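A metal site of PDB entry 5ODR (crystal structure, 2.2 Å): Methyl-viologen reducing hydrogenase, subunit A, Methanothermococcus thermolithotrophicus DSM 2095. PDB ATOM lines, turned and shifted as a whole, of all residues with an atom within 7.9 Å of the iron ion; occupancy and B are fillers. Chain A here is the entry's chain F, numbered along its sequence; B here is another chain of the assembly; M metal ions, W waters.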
ATOM      1  N   GLU A  42     -14.156  -7.301 -23.605  1.00  0.00           N
ATOM      2  CA  GLU A  42     -14.929  -6.649 -24.665  1.00  0.00           C
ATOM      3  C   GLU A  42     -14.395  -6.918 -26.060  1.00  0.00           C
ATOM      4  O   GLU A  42     -15.187  -7.066 -26.989  1.00  0.00           O
ATOM      5  CB  GLU A  42     -15.041  -5.137 -24.411  1.00  0.00           C
ATOM      6  CG  GLU A  42     -15.945  -4.822 -23.235  1.00  0.00           C
ATOM      7  CD  GLU A  42     -15.639  -3.519 -22.513  1.00  0.00           C
ATOM      8  OE1 GLU A  42     -14.454  -3.139 -22.425  1.00  0.00           O
ATOM      9  OE2 GLU A  42     -16.598  -2.918 -21.977  1.00  0.00           O
ATOM     10  N   GLU A 264     -18.354   6.954 -20.243  1.00  0.00           N
ATOM     11  CA  GLU A 264     -17.271   6.467 -19.397  1.00  0.00           C
ATOM     12  C   GLU A 264     -15.960   7.166 -19.739  1.00  0.00           C
ATOM     13  O   GLU A 264     -15.423   6.994 -20.830  1.00  0.00           O
ATOM     14  CB  GLU A 264     -17.109   4.954 -19.566  1.00  0.00           C
ATOM     15  CG  GLU A 264     -18.344   4.168 -19.183  1.00  0.00           C
ATOM     16  CD  GLU A 264     -18.165   2.667 -19.345  1.00  0.00           C
ATOM     17  OE1 GLU A 264     -17.840   2.000 -18.346  1.00  0.00           O
ATOM     18  OE2 GLU A 264     -18.310   2.167 -20.485  1.00  0.00           O
ATOM     19  N   LYS A 273     -12.449   2.886 -15.451  1.00  0.00           N
ATOM     20  CA  LYS A 273     -13.002   4.078 -16.063  1.00  0.00           C
ATOM     21  C   LYS A 273     -13.827   4.883 -15.068  1.00  0.00           C
ATOM     22  O   LYS A 273     -14.129   4.403 -13.981  1.00  0.00           O
ATOM     23  CB  LYS A 273     -13.811   3.716 -17.330  1.00  0.00           C
ATOM     24  CG  LYS A 273     -12.898   3.527 -18.539  1.00  0.00           C
ATOM     25  CD  LYS A 273     -13.267   2.358 -19.425  1.00  0.00           C
ATOM     26  CE  LYS A 273     -14.490   2.613 -20.254  1.00  0.00           C
ATOM     27  NZ  LYS A 273     -14.820   1.461 -21.125  1.00  0.00           N
ATOM     28  N   ILE A 379     -24.749  -3.991 -17.537  1.00  0.00           N
ATOM     29  CA  ILE A 379     -25.219  -3.962 -18.906  1.00  0.00           C
ATOM     30  C   ILE A 379     -24.257  -4.716 -19.812  1.00  0.00           C
ATOM     31  O   ILE A 379     -23.069  -4.425 -19.842  1.00  0.00           O
ATOM     32  CB  ILE A 379     -25.388  -2.498 -19.378  1.00  0.00           C
ATOM     33  CG1 ILE A 379     -26.611  -1.848 -18.713  1.00  0.00           C
ATOM     34  CG2 ILE A 379     -25.516  -2.415 -20.912  1.00  0.00           C
ATOM     35  CD1 ILE A 379     -26.497  -0.406 -18.550  1.00  0.00           C
ATOM     36  N   THR A 393     -18.764  -5.592 -28.749  1.00  0.00           N
ATOM     37  CA  THR A 393     -19.392  -5.724 -27.446  1.00  0.00           C
ATOM     38  C   THR A 393     -19.035  -4.551 -26.561  1.00  0.00           C
ATOM     39  O   THR A 393     -17.999  -3.911 -26.757  1.00  0.00           O
ATOM     40  CB  THR A 393     -18.978  -7.012 -26.674  1.00  0.00           C
ATOM     41  OG1 THR A 393     -17.710  -6.812 -26.068  1.00  0.00           O
ATOM     42  CG2 THR A 393     -18.947  -8.242 -27.536  1.00  0.00           C
ATOM     43  N   ASN A 394     -19.894  -4.279 -25.582  1.00  0.00           N
ATOM     44  CA  ASN A 394     -19.664  -3.212 -24.619  1.00  0.00           C
ATOM     45  C   ASN A 394     -20.221  -3.675 -23.306  1.00  0.00           C
ATOM     46  O   ASN A 394     -21.368  -4.126 -23.251  1.00  0.00           O
ATOM     47  CB  ASN A 394     -20.323  -1.902 -25.029  1.00  0.00           C
ATOM     48  CG  ASN A 394     -19.969  -0.771 -24.087  1.00  0.00           C
ATOM     49  OD1 ASN A 394     -18.850  -0.685 -23.559  1.00  0.00           O
ATOM     50  ND2 ASN A 394     -20.922   0.120 -23.834  1.00  0.00           N
ATOM     51  N   LEU A 395     -19.430  -3.588 -22.239  1.00  0.00           N
ATOM     52  CA  LEU A 395     -19.855  -3.997 -20.923  1.00  0.00           C
ATOM     53  C   LEU A 395     -19.714  -2.819 -19.946  1.00  0.00           C
ATOM     54  O   LEU A 395     -18.618  -2.274 -19.822  1.00  0.00           O
ATOM     55  CB  LEU A 395     -19.026  -5.186 -20.416  1.00  0.00           C
ATOM     56  CG  LEU A 395     -18.854  -6.370 -21.378  1.00  0.00           C
ATOM     57  CD1 LEU A 395     -17.813  -7.344 -20.849  1.00  0.00           C
ATOM     58  CD2 LEU A 395     -20.158  -7.099 -21.609  1.00  0.00           C
ATOM     59  N   VAL A 396     -20.807  -2.426 -19.297  1.00  0.00           N
ATOM     60  CA  VAL A 396     -20.819  -1.342 -18.299  1.00  0.00           C
ATOM     61  C   VAL A 396     -21.099  -2.158 -17.040  1.00  0.00           C
ATOM     62  O   VAL A 396     -22.248  -2.507 -16.757  1.00  0.00           O
ATOM     63  CB  VAL A 396     -21.906  -0.280 -18.573  1.00  0.00           C
ATOM     64  CG1 VAL A 396     -21.860   0.822 -17.517  1.00  0.00           C
ATOM     65  CG2 VAL A 396     -21.743   0.299 -19.971  1.00  0.00           C
ATOM     66  N   VAL A 397     -20.027  -2.492 -16.323  1.00  0.00           N
ATOM     67  CA  VAL A 397     -20.118  -3.352 -15.154  1.00  0.00           C
ATOM     68  C   VAL A 397     -20.079  -2.720 -13.775  1.00  0.00           C
ATOM     69  O   VAL A 397     -19.025  -2.336 -13.255  1.00  0.00           O
ATOM     70  CB  VAL A 397     -19.010  -4.430 -15.267  1.00  0.00           C
ATOM     71  CG1 VAL A 397     -19.144  -5.470 -14.162  1.00  0.00           C
ATOM     72  CG2 VAL A 397     -19.060  -5.103 -16.642  1.00  0.00           C
ATOM     73  N   VAL A 400     -17.739  -0.080 -11.790  1.00  0.00           N
ATOM     74  CA  VAL A 400     -17.103   1.007 -12.558  1.00  0.00           C
ATOM     75  C   VAL A 400     -17.816   2.324 -12.282  1.00  0.00           C
ATOM     76  O   VAL A 400     -17.178   3.368 -12.188  1.00  0.00           O
ATOM     77  CB  VAL A 400     -17.020   0.708 -14.085  1.00  0.00           C
ATOM     78  CG1 VAL A 400     -18.404   0.634 -14.725  1.00  0.00           C
ATOM     79  CG2 VAL A 400     -16.162   1.735 -14.809  1.00  0.00           C
ATOM     80  N   CYS A 445     -14.353  -7.266 -11.953  1.00  0.00           N
ATOM     81  CA  CYS A 445     -15.628  -7.024 -12.597  1.00  0.00           C
ATOM     82  C   CYS A 445     -15.664  -5.672 -13.293  1.00  0.00           C
ATOM     83  O   CYS A 445     -16.023  -5.570 -14.465  1.00  0.00           O
ATOM     84  CB  CYS A 445     -16.729  -7.099 -11.551  1.00  0.00           C
ATOM     85  SG  CYS A 445     -18.179  -8.035 -12.060  1.00  0.00           S
ATOM     86  N   ALA A 446     -15.299  -4.630 -12.554  1.00  0.00           N
ATOM     87  CA  ALA A 446     -15.312  -3.246 -13.028  1.00  0.00           C
ATOM     88  C   ALA A 446     -14.461  -2.973 -14.262  1.00  0.00           C
ATOM     89  O   ALA A 446     -14.845  -2.158 -15.090  1.00  0.00           O
ATOM     90  CB  ALA A 446     -14.900  -2.339 -11.891  1.00  0.00           C
ATOM     91  N   THR A 447     -13.301  -3.647 -14.378  1.00  0.00           N
ATOM     92  CA  THR A 447     -12.383  -3.465 -15.505  1.00  0.00           C
ATOM     93  C   THR A 447     -12.645  -4.445 -16.647  1.00  0.00           C
ATOM     94  O   THR A 447     -12.495  -4.071 -17.816  1.00  0.00           O
ATOM     95  CB  THR A 447     -10.945  -3.656 -15.015  1.00  0.00           C
ATOM     96  OG1 THR A 447     -10.818  -4.969 -14.459  1.00  0.00           O
ATOM     97  CG2 THR A 447     -10.548  -2.607 -14.002  1.00  0.00           C
ATOM     98  N   HIS A 448     -13.022  -5.692 -16.309  1.00  0.00           N
ATOM     99  CA  HIS A 448     -13.289  -6.760 -17.283  1.00  0.00           C
ATOM    100  C   HIS A 448     -12.307  -6.743 -18.468  1.00  0.00           C
ATOM    101  O   HIS A 448     -11.092  -6.890 -18.207  1.00  0.00           O
ATOM    102  CB  HIS A 448     -14.773  -6.757 -17.749  1.00  0.00           C
ATOM    103  CG  HIS A 448     -15.308  -5.389 -18.062  1.00  0.00           C
ATOM    104  ND1 HIS A 448     -15.754  -4.546 -17.068  1.00  0.00           N
ATOM    105  CD2 HIS A 448     -15.458  -4.777 -19.263  1.00  0.00           C
ATOM    106  CE1 HIS A 448     -16.160  -3.439 -17.681  1.00  0.00           C
ATOM    107  NE2 HIS A 448     -15.990  -3.531 -19.004  1.00  0.00           N
ATOM    108  N   LYS B 106      -9.984  -1.099 -27.463  1.00  0.00           N
ATOM    109  CA  LYS B 106     -11.419  -1.352 -27.363  1.00  0.00           C
ATOM    110  C   LYS B 106     -11.969  -0.915 -26.015  1.00  0.00           C
ATOM    111  O   LYS B 106     -12.970  -0.215 -25.950  1.00  0.00           O
ATOM    112  CB  LYS B 106     -11.715  -2.854 -27.571  1.00  0.00           C
ATOM    113  CG  LYS B 106     -13.180  -3.270 -27.340  1.00  0.00           C
ATOM    114  CD  LYS B 106     -14.180  -2.481 -28.184  1.00  0.00           C
ATOM    115  CE  LYS B 106     -14.014  -2.728 -29.665  1.00  0.00           C
ATOM    116  NZ  LYS B 106     -15.008  -1.979 -30.464  1.00  0.00           N
ATOM    117  N   ALA B 107     -11.308  -1.322 -24.936  1.00  0.00           N
ATOM    118  CA  ALA B 107     -11.741  -1.000 -23.590  1.00  0.00           C
ATOM    119  C   ALA B 107     -11.632   0.474 -23.225  1.00  0.00           C
ATOM    120  O   ALA B 107     -12.478   0.971 -22.484  1.00  0.00           O
ATOM    121  CB  ALA B 107     -10.949  -1.815 -22.578  1.00  0.00           C
ATOM    122  N   TYR B 108     -10.618   1.181 -23.741  1.00  0.00           N
ATOM    123  CA  TYR B 108     -10.435   2.593 -23.397  1.00  0.00           C
ATOM    124  C   TYR B 108     -10.667   3.606 -24.527  1.00  0.00           C
ATOM    125  O   TYR B 108     -10.395   4.783 -24.312  1.00  0.00           O
ATOM    126  CB  TYR B 108      -9.051   2.774 -22.763  1.00  0.00           C
ATOM    127  CG  TYR B 108      -8.920   1.840 -21.587  1.00  0.00           C
ATOM    128  CD1 TYR B 108      -9.655   2.040 -20.433  1.00  0.00           C
ATOM    129  CD2 TYR B 108      -8.153   0.682 -21.674  1.00  0.00           C
ATOM    130  CE1 TYR B 108      -9.589   1.150 -19.369  1.00  0.00           C
ATOM    131  CE2 TYR B 108      -8.074  -0.212 -20.608  1.00  0.00           C
ATOM    132  CZ  TYR B 108      -8.797   0.030 -19.458  1.00  0.00           C
ATOM    133  OH  TYR B 108      -8.727  -0.848 -18.398  1.00  0.00           O
ATOM    134  N   THR B 111     -15.157   1.498 -27.264  1.00  0.00           N
ATOM    135  CA  THR B 111     -16.409   0.959 -26.702  1.00  0.00           C
ATOM    136  C   THR B 111     -17.445   2.087 -26.871  1.00  0.00           C
ATOM    137  O   THR B 111     -17.102   3.251 -26.673  1.00  0.00           O
ATOM    138  CB  THR B 111     -16.235   0.474 -25.249  1.00  0.00           C
ATOM    139  OG1 THR B 111     -15.049   1.035 -24.685  1.00  0.00           O
ATOM    140  CG2 THR B 111     -16.184  -1.049 -25.161  1.00  0.00           C
ATOM    141  N   THR B 113     -19.853   3.477 -25.118  1.00  0.00           N
ATOM    142  CA  THR B 113     -20.043   4.449 -24.040  1.00  0.00           C
ATOM    143  C   THR B 113     -18.756   5.162 -23.623  1.00  0.00           C
ATOM    144  O   THR B 113     -18.825   6.092 -22.827  1.00  0.00           O
ATOM    145  CB  THR B 113     -20.702   3.795 -22.830  1.00  0.00           C
ATOM    146  OG1 THR B 113     -20.103   2.512 -22.620  1.00  0.00           O
ATOM    147  CG2 THR B 113     -22.188   3.658 -23.004  1.00  0.00           C
ATOM    148  N   THR B 114     -17.598   4.751 -24.150  1.00  0.00           N
ATOM    149  CA  THR B 114     -16.353   5.404 -23.765  1.00  0.00           C
ATOM    150  C   THR B 114     -16.161   6.779 -24.394  1.00  0.00           C
ATOM    151  O   THR B 114     -16.358   6.951 -25.600  1.00  0.00           O
ATOM    152  CB  THR B 114     -15.172   4.499 -24.055  1.00  0.00           C
ATOM    153  OG1 THR B 114     -15.343   3.302 -23.298  1.00  0.00           O
ATOM    154  CG2 THR B 114     -13.837   5.144 -23.700  1.00  0.00           C
HETATM  155 FE    FE M   1     -16.655  -1.795 -20.146  1.00  0.00          FE
HETATM  156  O   HOH W   1     -14.618  -1.283 -20.533  1.00  0.00           O
HETATM  157  O   HOH W   2     -16.753  -0.448 -18.403  1.00  0.00           O
HETATM  158  O   HOH W   3     -17.286  -0.057 -21.479  1.00  0.00           O
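ND1 of His 448 sits at hydrogen-bond distance from O of Cys 445, at 2.8 Å. NZ of Lys 273 is in salt-bridge range of OE2 of Glu 264. A ring nitrogen (ND1) of His 448 lies close to the backbone carbonyl oxygen of Ala 446 (3.2 Å). The backbone carbonyl oxygen of Glu 42 sits at hydrogen-bond distance from the side-chain hydroxyl of Thr 393, 2.7 Å away. O of Ala 107 of chain B is in hydrogen-bond range of NZ of Lys 273, 2.8 Å away. The side-chain hydroxyl of Thr 114 of chain B is in hydrogen-bond range of the side-chain amino group of Lys 273 (2.9 Å).
Lys 273 touches the iron ion (NZ to FE, 3.9 Å). The nearest printed residue that does not touch the iron ion is Asn 394 (4.2 Å).
The iron ion is bound by the backbone carbonyl oxygen (O) of Leu 395 (2.0 Å), water W1 (2.1 Å), the side-chain carboxylate (OE2) of Glu 42 (2.1 Å), a ring nitrogen (NE2) of His 448 (2.2 Å), water W2 (2.2 Å) and water W3 (2.3 Å).
Water W3 lies within hydrogen-bond range of OE2 of Glu 264 (2.6 Å), OD1 of Asn 394 (2.7 Å) and NZ of Lys 273 (2.9 Å). Water W1 lies within hydrogen-bond range of the side-chain carboxylate of Glu 42 (2.7 Å) and the side-chain amino group of Lys 273 (2.8 Å).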
